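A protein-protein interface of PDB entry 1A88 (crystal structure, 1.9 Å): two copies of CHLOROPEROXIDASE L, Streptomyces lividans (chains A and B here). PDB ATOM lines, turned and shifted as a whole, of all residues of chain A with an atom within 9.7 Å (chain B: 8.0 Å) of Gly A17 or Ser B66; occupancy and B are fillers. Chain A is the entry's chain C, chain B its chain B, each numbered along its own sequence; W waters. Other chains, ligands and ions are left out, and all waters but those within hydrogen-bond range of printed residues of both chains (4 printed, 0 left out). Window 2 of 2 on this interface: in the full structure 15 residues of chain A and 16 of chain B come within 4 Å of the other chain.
No position is printed for both chains. Of the 8 pairs that touch across the chains among the printed residues, none has its exchanged pair printed and touching as well.
The side-chain amide oxygen of Gln B64 lies within hydrogen-bond range of the side-chain amino group of Lys A14, 2.8 Å away. The backbone NH (N) of Gly A17 sits at hydrogen-bond distance from the side-chain hydroxyl (OG) of Ser B66 (2.8 Å). NE1 of Trp A16 is in hydrogen-bond range of O of Gln B64.
Of the printed residues of chain B, Lys A14 touches Gln B64. Of the printed residues of chain B, Asp A15 touches Ser B66 (3.7 Å). Printed residues of chain B within 4 Å of Trp A16: Gln B64 (2.9 Å), Pro B65 (3.9 Å), Ser B66 (3.6 Å) and Asn B193 (3.2 Å). No residue of chain B comes within 4 Å of Pro A18. Printed residues of chain B within 4 Å of Leu A42: Asn B193. Arg B57 touches none of the printed residues of chain A. Of the printed residues of chain A, Gln B64 touches Lys A14 and Trp A16. Of the printed residues of chain A, Pro B65 touches Trp A16. Of chain A, only Asp A15 (3.7 Å), Trp A16 (3.6 Å) and Gly A17 (2.8 Å) come within 4 Å of Ser B66. The nearest residue of chain A that does not touch Ser B66 is Arg A19 (4.2 Å).
Water W4 lies within hydrogen-bond range of the backbone carbonyl oxygen of Gly A17 (2.6 Å), the side-chain hydroxyl of Ser B66 (2.9 Å) and the guanidinium group of Arg A19 (3.4 Å). Water W2 bridges the backbone carbonyl oxygen (O) of Gln B64 (2.9 Å) and the backbone NH (N) of Asp A15 (2.9 Å). Water W3 bridges N of Gln B64 (2.9 Å) and N of Gly A1 (3.3 Å). Water W1 bridges NE2 of Gln B64 and NZ of Lys A14.
Asp A15 touches Ser B66. Pro B65 touches Trp A16 (O to CD1, 3.9 Å). Trp A16 touches Ser B66. Trp A16 touches Asn B193. CA of Asn B193 touches CD2 of Leu A42 (3.8 Å).
Printed residues of chain A that touch a printed residue of chain B: Lys A14, Asp A15, Trp A16, Gly A17 and Leu A42. Of the 13 printed residues of chain B, 4 touch a printed residue of chain A. Printed residues of chain B that touch a printed residue of chain A: Gln B64, Pro B65, Ser B66 and Asn B193.
The backbone carbonyl oxygen (O) of Pro B65 is in hydrogen-bond range of a ring nitrogen (NE2) of His B69 (3.1 Å). NH2 of Arg A50 lies within salt-bridge range of OD2 of Asp A15 (2.8 Å). The backbone carbonyl oxygen (O) of Val A51 is in hydrogen-bond range of the backbone NH (N) of Trp A16 (2.8 Å). The backbone carbonyl oxygen (O) of Pro B65 sits at hydrogen-bond distance from the side-chain amide nitrogen (ND2) of Asn B193 (3.3 Å). The backbone carbonyl oxygen (O) of Gly A17 lies within hydrogen-bond range of the guanidinium group (NH2) of Arg A19, at 2.8 Å. The side-chain carboxylate of Asp A15 lies within salt-bridge range of the guanidinium group of Arg A19 (2.9 Å).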
ATOM      1  N   GLY A   1     -22.927 -16.125  23.370  1.00  0.00           N
ATOM      2  CA  GLY A   1     -23.879 -14.959  23.381  1.00  0.00           C
ATOM      3  C   GLY A   1     -24.238 -14.660  21.934  1.00  0.00           C
ATOM      4  O   GLY A   1     -23.572 -15.079  20.980  1.00  0.00           O
ATOM      5  N   TYR A  13     -21.103 -14.956  19.457  1.00  0.00           N
ATOM      6  CA  TYR A  13     -19.769 -14.561  19.936  1.00  0.00           C
ATOM      7  C   TYR A  13     -19.500 -15.327  21.226  1.00  0.00           C
ATOM      8  O   TYR A  13     -20.396 -15.833  21.903  1.00  0.00           O
ATOM      9  CB  TYR A  13     -19.638 -13.030  20.089  1.00  0.00           C
ATOM     10  CG  TYR A  13     -20.487 -12.491  21.208  1.00  0.00           C
ATOM     11  CD1 TYR A  13     -21.799 -12.109  21.064  1.00  0.00           C
ATOM     12  CD2 TYR A  13     -19.922 -12.403  22.492  1.00  0.00           C
ATOM     13  CE1 TYR A  13     -22.569 -11.636  22.128  1.00  0.00           C
ATOM     14  CE2 TYR A  13     -20.652 -11.953  23.566  1.00  0.00           C
ATOM     15  CZ  TYR A  13     -21.980 -11.584  23.379  1.00  0.00           C
ATOM     16  OH  TYR A  13     -22.703 -11.161  24.457  1.00  0.00           O
ATOM     17  N   LYS A  14     -18.220 -15.400  21.575  1.00  0.00           N
ATOM     18  CA  LYS A  14     -17.762 -16.001  22.837  1.00  0.00           C
ATOM     19  C   LYS A  14     -17.143 -14.831  23.650  1.00  0.00           C
ATOM     20  O   LYS A  14     -16.505 -13.972  23.009  1.00  0.00           O
ATOM     21  CB  LYS A  14     -16.551 -16.883  22.483  1.00  0.00           C
ATOM     22  CG  LYS A  14     -16.862 -18.286  22.041  1.00  0.00           C
ATOM     23  CD  LYS A  14     -15.589 -18.860  21.430  1.00  0.00           C
ATOM     24  CE  LYS A  14     -15.965 -19.819  20.315  1.00  0.00           C
ATOM     25  NZ  LYS A  14     -15.665 -21.211  20.811  1.00  0.00           N
ATOM     26  N   ASP A  15     -17.264 -14.886  24.948  1.00  0.00           N
ATOM     27  CA  ASP A  15     -16.705 -13.847  25.834  1.00  0.00           C
ATOM     28  C   ASP A  15     -16.256 -14.550  27.094  1.00  0.00           C
ATOM     29  O   ASP A  15     -17.069 -14.975  27.941  1.00  0.00           O
ATOM     30  CB  ASP A  15     -17.792 -12.824  26.180  1.00  0.00           C
ATOM     31  CG  ASP A  15     -17.359 -11.699  27.095  1.00  0.00           C
ATOM     32  OD1 ASP A  15     -16.175 -11.689  27.506  1.00  0.00           O
ATOM     33  OD2 ASP A  15     -18.253 -10.862  27.412  1.00  0.00           O
ATOM     34  N   TRP A  16     -14.934 -14.816  27.210  1.00  0.00           N
ATOM     35  CA  TRP A  16     -14.490 -15.596  28.370  1.00  0.00           C
ATOM     36  C   TRP A  16     -13.452 -14.773  29.173  1.00  0.00           C
ATOM     37  O   TRP A  16     -12.866 -13.864  28.638  1.00  0.00           O
ATOM     38  CB  TRP A  16     -13.795 -16.869  27.889  1.00  0.00           C
ATOM     39  CG  TRP A  16     -14.627 -17.813  27.038  1.00  0.00           C
ATOM     40  CD1 TRP A  16     -15.975 -17.984  27.100  1.00  0.00           C
ATOM     41  CD2 TRP A  16     -14.143 -18.730  26.062  1.00  0.00           C
ATOM     42  NE1 TRP A  16     -16.376 -18.955  26.192  1.00  0.00           N
ATOM     43  CE2 TRP A  16     -15.261 -19.448  25.563  1.00  0.00           C
ATOM     44  CE3 TRP A  16     -12.867 -19.096  25.613  1.00  0.00           C
ATOM     45  CZ2 TRP A  16     -15.156 -20.452  24.607  1.00  0.00           C
ATOM     46  CZ3 TRP A  16     -12.742 -20.081  24.647  1.00  0.00           C
ATOM     47  CH2 TRP A  16     -13.887 -20.747  24.143  1.00  0.00           C
ATOM     48  N   GLY A  17     -13.302 -15.125  30.451  1.00  0.00           N
ATOM     49  CA  GLY A  17     -12.279 -14.453  31.273  1.00  0.00           C
ATOM     50  C   GLY A  17     -12.899 -13.436  32.217  1.00  0.00           C
ATOM     51  O   GLY A  17     -14.101 -13.142  32.245  1.00  0.00           O
ATOM     52  N   PRO A  18     -12.004 -12.847  33.036  1.00  0.00           N
ATOM     53  CA  PRO A  18     -12.388 -11.825  33.986  1.00  0.00           C
ATOM     54  C   PRO A  18     -13.118 -10.680  33.335  1.00  0.00           C
ATOM     55  O   PRO A  18     -12.691 -10.043  32.348  1.00  0.00           O
ATOM     56  CB  PRO A  18     -11.047 -11.298  34.546  1.00  0.00           C
ATOM     57  CG  PRO A  18      -9.997 -12.267  34.142  1.00  0.00           C
ATOM     58  CD  PRO A  18     -10.563 -13.136  33.056  1.00  0.00           C
ATOM     59  N   ARG A  19     -14.166 -10.243  34.018  1.00  0.00           N
ATOM     60  CA  ARG A  19     -14.912  -9.069  33.557  1.00  0.00           C
ATOM     61  C   ARG A  19     -14.125  -7.774  33.574  1.00  0.00           C
ATOM     62  O   ARG A  19     -14.485  -6.866  32.829  1.00  0.00           O
ATOM     63  CB  ARG A  19     -16.180  -8.926  34.401  1.00  0.00           C
ATOM     64  CG  ARG A  19     -16.916 -10.279  34.513  1.00  0.00           C
ATOM     65  CD  ARG A  19     -17.447 -10.693  33.151  1.00  0.00           C
ATOM     66  NE  ARG A  19     -16.572 -11.517  32.330  1.00  0.00           N
ATOM     67  CZ  ARG A  19     -16.706 -11.625  30.998  1.00  0.00           C
ATOM     68  NH1 ARG A  19     -17.692 -10.887  30.440  1.00  0.00           N
ATOM     69  NH2 ARG A  19     -15.914 -12.417  30.293  1.00  0.00           N
ATOM     70  N   ASP A  20     -13.093  -7.670  34.392  1.00  0.00           N
ATOM     71  CA  ASP A  20     -12.284  -6.459  34.458  1.00  0.00           C
ATOM     72  C   ASP A  20     -10.925  -6.650  33.782  1.00  0.00           C
ATOM     73  O   ASP A  20      -9.972  -5.893  33.994  1.00  0.00           O
ATOM     74  CB  ASP A  20     -12.085  -6.086  35.931  1.00  0.00           C
ATOM     75  CG  ASP A  20     -11.248  -7.081  36.703  1.00  0.00           C
ATOM     76  OD1 ASP A  20     -11.261  -8.313  36.437  1.00  0.00           O
ATOM     77  OD2 ASP A  20     -10.549  -6.617  37.641  1.00  0.00           O
ATOM     78  N   GLY A  21     -10.806  -7.714  32.997  1.00  0.00           N
ATOM     79  CA  GLY A  21      -9.601  -8.017  32.227  1.00  0.00           C
ATOM     80  C   GLY A  21      -9.569  -7.111  31.010  1.00  0.00           C
ATOM     81  O   GLY A  21     -10.630  -6.653  30.552  1.00  0.00           O
ATOM     82  N   LEU A  22      -8.419  -6.720  30.467  1.00  0.00           N
ATOM     83  CA  LEU A  22      -8.341  -5.903  29.298  1.00  0.00           C
ATOM     84  C   LEU A  22      -8.904  -6.818  28.157  1.00  0.00           C
ATOM     85  O   LEU A  22      -8.516  -7.984  28.060  1.00  0.00           O
ATOM     86  CB  LEU A  22      -6.897  -5.628  28.976  1.00  0.00           C
ATOM     87  CG  LEU A  22      -6.465  -4.785  27.797  1.00  0.00           C
ATOM     88  CD1 LEU A  22      -5.025  -4.288  27.966  1.00  0.00           C
ATOM     89  CD2 LEU A  22      -6.431  -5.683  26.558  1.00  0.00           C
ATOM     90  N   PRO A  23      -9.764  -6.272  27.335  1.00  0.00           N
ATOM     91  CA  PRO A  23     -10.434  -7.091  26.282  1.00  0.00           C
ATOM     92  C   PRO A  23      -9.602  -7.260  25.054  1.00  0.00           C
ATOM     93  O   PRO A  23      -9.140  -6.303  24.431  1.00  0.00           O
ATOM     94  CB  PRO A  23     -11.718  -6.339  25.968  1.00  0.00           C
ATOM     95  CG  PRO A  23     -11.696  -5.071  26.721  1.00  0.00           C
ATOM     96  CD  PRO A  23     -10.391  -4.938  27.455  1.00  0.00           C
ATOM     97  N   VAL A  24      -9.281  -8.524  24.677  1.00  0.00           N
ATOM     98  CA  VAL A  24      -8.565  -8.888  23.482  1.00  0.00           C
ATOM     99  C   VAL A  24      -9.614  -9.591  22.542  1.00  0.00           C
ATOM    100  O   VAL A  24     -10.274 -10.552  22.958  1.00  0.00           O
ATOM    101  CB  VAL A  24      -7.420  -9.893  23.810  1.00  0.00           C
ATOM    102  CG1 VAL A  24      -6.694 -10.206  22.525  1.00  0.00           C
ATOM    103  CG2 VAL A  24      -6.441  -9.289  24.849  1.00  0.00           C
ATOM    104  N   MET A  41      -7.024 -17.994  22.290  1.00  0.00           N
ATOM    105  CA  MET A  41      -7.905 -17.711  23.411  1.00  0.00           C
ATOM    106  C   MET A  41      -7.501 -18.335  24.734  1.00  0.00           C
ATOM    107  O   MET A  41      -7.504 -17.611  25.770  1.00  0.00           O
ATOM    108  CB  MET A  41      -9.372 -18.171  23.073  1.00  0.00           C
ATOM    109  CG  MET A  41      -9.757 -17.047  22.044  1.00  0.00           C
ATOM    110  SD  MET A  41     -11.418 -17.223  21.486  1.00  0.00           S
ATOM    111  CE  MET A  41     -12.477 -16.748  22.821  1.00  0.00           C
ATOM    112  N   LEU A  42      -7.124 -19.628  24.720  1.00  0.00           N
ATOM    113  CA  LEU A  42      -6.675 -20.253  25.989  1.00  0.00           C
ATOM    114  C   LEU A  42      -5.344 -19.642  26.452  1.00  0.00           C
ATOM    115  O   LEU A  42      -5.187 -19.461  27.673  1.00  0.00           O
ATOM    116  CB  LEU A  42      -6.524 -21.765  25.846  1.00  0.00           C
ATOM    117  CG  LEU A  42      -7.858 -22.534  25.641  1.00  0.00           C
ATOM    118  CD1 LEU A  42      -7.612 -24.042  25.659  1.00  0.00           C
ATOM    119  CD2 LEU A  42      -8.881 -22.163  26.683  1.00  0.00           C
ATOM    120  N   PHE A  44      -4.196 -16.431  25.985  1.00  0.00           N
ATOM    121  CA  PHE A  44      -4.442 -15.127  26.649  1.00  0.00           C
ATOM    122  C   PHE A  44      -5.256 -15.274  27.890  1.00  0.00           C
ATOM    123  O   PHE A  44      -5.028 -14.524  28.857  1.00  0.00           O
ATOM    124  CB  PHE A  44      -5.087 -14.110  25.711  1.00  0.00           C
ATOM    125  CG  PHE A  44      -4.067 -13.475  24.812  1.00  0.00           C
ATOM    126  CD1 PHE A  44      -3.421 -12.314  25.258  1.00  0.00           C
ATOM    127  CD2 PHE A  44      -3.739 -13.993  23.596  1.00  0.00           C
ATOM    128  CE1 PHE A  44      -2.501 -11.703  24.449  1.00  0.00           C
ATOM    129  CE2 PHE A  44      -2.769 -13.406  22.805  1.00  0.00           C
ATOM    130  CZ  PHE A  44      -2.153 -12.228  23.219  1.00  0.00           C
ATOM    131  N   LEU A  45      -6.207 -16.226  27.958  1.00  0.00           N
ATOM    132  CA  LEU A  45      -6.948 -16.408  29.199  1.00  0.00           C
ATOM    133  C   LEU A  45      -6.009 -16.823  30.331  1.00  0.00           C
ATOM    134  O   LEU A  45      -6.215 -16.399  31.471  1.00  0.00           O
ATOM    135  CB  LEU A  45      -7.923 -17.566  29.061  1.00  0.00           C
ATOM    136  CG  LEU A  45      -9.378 -17.332  28.730  1.00  0.00           C
ATOM    137  CD1 LEU A  45     -10.068 -18.716  28.613  1.00  0.00           C
ATOM    138  CD2 LEU A  45     -10.036 -16.457  29.759  1.00  0.00           C
ATOM    139  N   SER A  46      -5.024 -17.646  30.008  1.00  0.00           N
ATOM    140  CA  SER A  46      -4.071 -18.072  31.028  1.00  0.00           C
ATOM    141  C   SER A  46      -3.246 -16.874  31.542  1.00  0.00           C
ATOM    142  O   SER A  46      -2.799 -16.970  32.689  1.00  0.00           O
ATOM    143  CB  SER A  46      -3.218 -19.219  30.503  1.00  0.00           C
ATOM    144  OG  SER A  46      -2.207 -18.748  29.641  1.00  0.00           O
ATOM    145  N   HIS A  47      -3.092 -15.770  30.863  1.00  0.00           N
ATOM    146  CA  HIS A  47      -2.414 -14.567  31.325  1.00  0.00           C
ATOM    147  C   HIS A  47      -3.359 -13.517  31.888  1.00  0.00           C
ATOM    148  O   HIS A  47      -2.900 -12.395  32.165  1.00  0.00           O
ATOM    149  CB  HIS A  47      -1.597 -13.966  30.175  1.00  0.00           C
ATOM    150  CG  HIS A  47      -0.392 -14.825  29.856  1.00  0.00           C
ATOM    151  ND1 HIS A  47       0.798 -14.682  30.540  1.00  0.00           N
ATOM    152  CD2 HIS A  47      -0.199 -15.825  28.956  1.00  0.00           C
ATOM    153  CE1 HIS A  47       1.668 -15.554  30.070  1.00  0.00           C
ATOM    154  NE2 HIS A  47       1.101 -16.242  29.112  1.00  0.00           N
ATOM    155  N   GLY A  48      -4.587 -13.862  32.242  1.00  0.00           N
ATOM    156  CA  GLY A  48      -5.535 -13.004  32.884  1.00  0.00           C
ATOM    157  C   GLY A  48      -6.330 -12.074  31.986  1.00  0.00           C
ATOM    158  O   GLY A  48      -7.021 -11.223  32.531  1.00  0.00           O
ATOM    159  N   TYR A  49      -6.281 -12.192  30.665  1.00  0.00           N
ATOM    160  CA  TYR A  49      -7.065 -11.295  29.818  1.00  0.00           C
ATOM    161  C   TYR A  49      -8.503 -11.802  29.621  1.00  0.00           C
ATOM    162  O   TYR A  49      -8.815 -12.956  29.816  1.00  0.00           O
ATOM    163  CB  TYR A  49      -6.426 -11.263  28.415  1.00  0.00           C
ATOM    164  CG  TYR A  49      -5.066 -10.560  28.525  1.00  0.00           C
ATOM    165  CD1 TYR A  49      -4.987  -9.186  28.420  1.00  0.00           C
ATOM    166  CD2 TYR A  49      -3.894 -11.308  28.758  1.00  0.00           C
ATOM    167  CE1 TYR A  49      -3.768  -8.519  28.555  1.00  0.00           C
ATOM    168  CE2 TYR A  49      -2.691 -10.648  28.886  1.00  0.00           C
ATOM    169  CZ  TYR A  49      -2.621  -9.282  28.799  1.00  0.00           C
ATOM    170  OH  TYR A  49      -1.410  -8.628  28.930  1.00  0.00           O
ATOM    171  N   ARG A  50      -9.353 -10.855  29.217  1.00  0.00           N
ATOM    172  CA  ARG A  50     -10.726 -11.228  28.834  1.00  0.00           C
ATOM    173  C   ARG A  50     -10.590 -11.472  27.335  1.00  0.00           C
ATOM    174  O   ARG A  50      -9.967 -10.646  26.662  1.00  0.00           O
ATOM    175  CB  ARG A  50     -11.650 -10.051  29.079  1.00  0.00           C
ATOM    176  CG  ARG A  50     -13.094 -10.308  28.502  1.00  0.00           C
ATOM    177  CD  ARG A  50     -13.898  -9.071  28.989  1.00  0.00           C
ATOM    178  NE  ARG A  50     -15.266  -9.181  28.472  1.00  0.00           N
ATOM    179  CZ  ARG A  50     -16.114  -8.145  28.516  1.00  0.00           C
ATOM    180  NH1 ARG A  50     -15.699  -6.971  29.010  1.00  0.00           N
ATOM    181  NH2 ARG A  50     -17.341  -8.289  28.032  1.00  0.00           N
ATOM    182  N   VAL A  51     -11.110 -12.554  26.775  1.00  0.00           N
ATOM    183  CA  VAL A  51     -10.969 -12.820  25.360  1.00  0.00           C
ATOM    184  C   VAL A  51     -12.350 -12.968  24.706  1.00  0.00           C
ATOM    185  O   VAL A  51     -13.261 -13.595  25.262  1.00  0.00           O
ATOM    186  CB  VAL A  51     -10.116 -14.115  25.121  1.00  0.00           C
ATOM    187  CG1 VAL A  51      -8.682 -13.843  25.634  1.00  0.00           C
ATOM    188  CG2 VAL A  51     -10.709 -15.318  25.783  1.00  0.00           C
ATOM    189  N   ILE A  52     -12.510 -12.373  23.560  1.00  0.00           N
ATOM    190  CA  ILE A  52     -13.778 -12.232  22.849  1.00  0.00           C
ATOM    191  C   ILE A  52     -13.603 -12.616  21.401  1.00  0.00           C
ATOM    192  O   ILE A  52     -12.669 -12.136  20.756  1.00  0.00           O
ATOM    193  CB  ILE A  52     -14.250 -10.746  22.887  1.00  0.00           C
ATOM    194  CG1 ILE A  52     -14.558 -10.392  24.366  1.00  0.00           C
ATOM    195  CG2 ILE A  52     -15.536 -10.507  22.071  1.00  0.00           C
ATOM    196  CD1 ILE A  52     -14.781  -8.929  24.672  1.00  0.00           C
ATOM    197  N   ASP B   7     -27.486 -18.786  36.399  1.00  0.00           N
ATOM    198  CA  ASP B   7     -26.575 -17.766  35.925  1.00  0.00           C
ATOM    199  C   ASP B   7     -26.877 -17.352  34.486  1.00  0.00           C
ATOM    200  O   ASP B   7     -26.060 -16.641  33.876  1.00  0.00           O
ATOM    201  CB  ASP B   7     -25.120 -18.188  36.094  1.00  0.00           C
ATOM    202  CG  ASP B   7     -24.719 -19.363  35.200  1.00  0.00           C
ATOM    203  OD1 ASP B   7     -25.574 -19.969  34.518  1.00  0.00           O
ATOM    204  OD2 ASP B   7     -23.503 -19.645  35.161  1.00  0.00           O
ATOM    205  N   THR B   9     -27.119 -19.345  31.745  1.00  0.00           N
ATOM    206  CA  THR B   9     -26.667 -20.275  30.719  1.00  0.00           C
ATOM    207  C   THR B   9     -27.804 -21.091  30.096  1.00  0.00           C
ATOM    208  O   THR B   9     -28.610 -21.664  30.819  1.00  0.00           O
ATOM    209  CB  THR B   9     -25.667 -21.290  31.337  1.00  0.00           C
ATOM    210  OG1 THR B   9     -24.573 -20.500  31.874  1.00  0.00           O
ATOM    211  CG2 THR B   9     -25.076 -22.225  30.284  1.00  0.00           C
ATOM    212  N   ARG B  57     -22.895 -27.709  30.059  1.00  0.00           N
ATOM    213  CA  ARG B  57     -22.523 -26.344  29.700  1.00  0.00           C
ATOM    214  C   ARG B  57     -21.159 -26.353  29.019  1.00  0.00           C
ATOM    215  O   ARG B  57     -20.352 -27.207  29.356  1.00  0.00           O
ATOM    216  CB  ARG B  57     -22.527 -25.376  30.858  1.00  0.00           C
ATOM    217  CG  ARG B  57     -21.646 -25.725  32.052  1.00  0.00           C
ATOM    218  CD  ARG B  57     -21.485 -24.535  33.016  1.00  0.00           C
ATOM    219  NE  ARG B  57     -22.776 -24.191  33.656  1.00  0.00           N
ATOM    220  CZ  ARG B  57     -23.135 -22.963  34.015  1.00  0.00           C
ATOM    221  NH1 ARG B  57     -22.386 -21.873  33.872  1.00  0.00           N
ATOM    222  NH2 ARG B  57     -24.347 -22.778  34.564  1.00  0.00           N
ATOM    223  N   ASP B  63     -24.716 -23.332  25.493  1.00  0.00           N
ATOM    224  CA  ASP B  63     -23.957 -22.094  25.538  1.00  0.00           C
ATOM    225  C   ASP B  63     -22.528 -22.375  25.996  1.00  0.00           C
ATOM    226  O   ASP B  63     -22.288 -23.372  26.677  1.00  0.00           O
ATOM    227  CB  ASP B  63     -24.501 -21.118  26.613  1.00  0.00           C
ATOM    228  CG  ASP B  63     -25.768 -20.385  26.175  1.00  0.00           C
ATOM    229  OD1 ASP B  63     -26.152 -20.497  24.993  1.00  0.00           O
ATOM    230  OD2 ASP B  63     -26.443 -19.811  27.054  1.00  0.00           O
ATOM    231  N   GLN B  64     -21.630 -21.441  25.751  1.00  0.00           N
ATOM    232  CA  GLN B  64     -20.203 -21.550  26.131  1.00  0.00           C
ATOM    233  C   GLN B  64     -19.880 -20.425  27.119  1.00  0.00           C
ATOM    234  O   GLN B  64     -19.218 -19.446  26.730  1.00  0.00           O
ATOM    235  CB  GLN B  64     -19.421 -21.390  24.827  1.00  0.00           C
ATOM    236  CG  GLN B  64     -19.730 -22.536  23.827  1.00  0.00           C
ATOM    237  CD  GLN B  64     -18.699 -22.626  22.716  1.00  0.00           C
ATOM    238  OE1 GLN B  64     -17.808 -21.798  22.490  1.00  0.00           O
ATOM    239  NE2 GLN B  64     -18.791 -23.673  21.897  1.00  0.00           N
ATOM    240  N   PRO B  65     -20.257 -20.575  28.366  1.00  0.00           N
ATOM    241  CA  PRO B  65     -20.051 -19.497  29.349  1.00  0.00           C
ATOM    242  C   PRO B  65     -18.620 -19.359  29.812  1.00  0.00           C
ATOM    243  O   PRO B  65     -17.775 -20.261  29.676  1.00  0.00           O
ATOM    244  CB  PRO B  65     -21.049 -19.842  30.448  1.00  0.00           C
ATOM    245  CG  PRO B  65     -21.074 -21.343  30.461  1.00  0.00           C
ATOM    246  CD  PRO B  65     -20.961 -21.720  28.979  1.00  0.00           C
ATOM    247  N   SER B  66     -18.294 -18.222  30.404  1.00  0.00           N
ATOM    248  CA  SER B  66     -16.945 -18.009  30.928  1.00  0.00           C
ATOM    249  C   SER B  66     -16.730 -18.869  32.159  1.00  0.00           C
ATOM    250  O   SER B  66     -15.623 -19.403  32.351  1.00  0.00           O
ATOM    251  CB  SER B  66     -16.746 -16.521  31.255  1.00  0.00           C
ATOM    252  OG  SER B  66     -15.429 -16.360  31.789  1.00  0.00           O
ATOM    253  N   THR B  67     -17.741 -19.084  33.015  1.00  0.00           N
ATOM    254  CA  THR B  67     -17.558 -19.836  34.234  1.00  0.00           C
ATOM    255  C   THR B  67     -18.554 -20.959  34.459  1.00  0.00           C
ATOM    256  O   THR B  67     -19.462 -21.233  33.664  1.00  0.00           O
ATOM    257  CB  THR B  67     -17.666 -18.923  35.502  1.00  0.00           C
ATOM    258  OG1 THR B  67     -19.003 -18.369  35.541  1.00  0.00           O
ATOM    259  CG2 THR B  67     -16.734 -17.744  35.512  1.00  0.00           C
ATOM    260  N   GLY B  68     -18.353 -21.630  35.613  1.00  0.00           N
ATOM    261  CA  GLY B  68     -19.204 -22.727  36.048  1.00  0.00           C
ATOM    262  C   GLY B  68     -18.670 -24.071  35.584  1.00  0.00           C
ATOM    263  O   GLY B  68     -19.418 -25.039  35.620  1.00  0.00           O
ATOM    264  N   HIS B  69     -17.368 -24.182  35.227  1.00  0.00           N
ATOM    265  CA  HIS B  69     -16.906 -25.496  34.777  1.00  0.00           C
ATOM    266  C   HIS B  69     -16.454 -26.354  35.946  1.00  0.00           C
ATOM    267  O   HIS B  69     -15.228 -26.580  36.090  1.00  0.00           O
ATOM    268  CB  HIS B  69     -15.794 -25.311  33.748  1.00  0.00           C
ATOM    269  CG  HIS B  69     -16.269 -24.342  32.705  1.00  0.00           C
ATOM    270  ND1 HIS B  69     -17.317 -24.694  31.854  1.00  0.00           N
ATOM    271  CD2 HIS B  69     -15.899 -23.078  32.415  1.00  0.00           C
ATOM    272  CE1 HIS B  69     -17.556 -23.650  31.070  1.00  0.00           C
ATOM    273  NE2 HIS B  69     -16.700 -22.700  31.349  1.00  0.00           N
ATOM    274  N   ASN B 193     -12.455 -23.623  26.418  1.00  0.00           N
ATOM    275  CA  ASN B 193     -12.258 -23.362  27.854  1.00  0.00           C
ATOM    276  C   ASN B 193     -12.994 -24.360  28.736  1.00  0.00           C
ATOM    277  O   ASN B 193     -12.381 -24.833  29.689  1.00  0.00           O
ATOM    278  CB  ASN B 193     -12.618 -21.919  28.213  1.00  0.00           C
ATOM    279  CG  ASN B 193     -14.124 -21.665  28.111  1.00  0.00           C
ATOM    280  OD1 ASN B 193     -14.872 -22.239  27.286  1.00  0.00           O
ATOM    281  ND2 ASN B 193     -14.573 -20.790  29.017  1.00  0.00           N
ATOM    282  N   ALA B 194     -14.211 -24.778  28.402  1.00  0.00           N
ATOM    283  CA  ALA B 194     -14.933 -25.736  29.249  1.00  0.00           C
ATOM    284  C   ALA B 194     -14.216 -27.080  29.233  1.00  0.00           C
ATOM    285  O   ALA B 194     -14.106 -27.734  30.258  1.00  0.00           O
ATOM    286  CB  ALA B 194     -16.368 -25.972  28.758  1.00  0.00           C
ATOM    287  N   GLU B 197     -10.960 -26.779  31.368  1.00  0.00           N
ATOM    288  CA  GLU B 197     -11.260 -26.736  32.807  1.00  0.00           C
ATOM    289  C   GLU B 197     -11.898 -27.967  33.380  1.00  0.00           C
ATOM    290  O   GLU B 197     -11.674 -28.343  34.549  1.00  0.00           O
ATOM    291  CB  GLU B 197     -12.202 -25.519  33.087  1.00  0.00           C
ATOM    292  CG  GLU B 197     -11.435 -24.243  32.760  1.00  0.00           C
ATOM    293  CD  GLU B 197     -12.033 -23.011  33.397  1.00  0.00           C
ATOM    294  OE1 GLU B 197     -12.582 -23.042  34.535  1.00  0.00           O
ATOM    295  OE2 GLU B 197     -11.983 -21.920  32.768  1.00  0.00           O
HETATM  296  O   HOH W   1     -16.403 -24.354  20.056  1.00  0.00           O
HETATM  297  O   HOH W   2     -19.363 -16.714  25.822  1.00  0.00           O
HETATM  298  O   HOH W   3     -22.679 -19.308  24.026  1.00  0.00           O
HETATM  299  O   HOH W   4     -15.742 -14.385  33.903  1.00  0.00           O
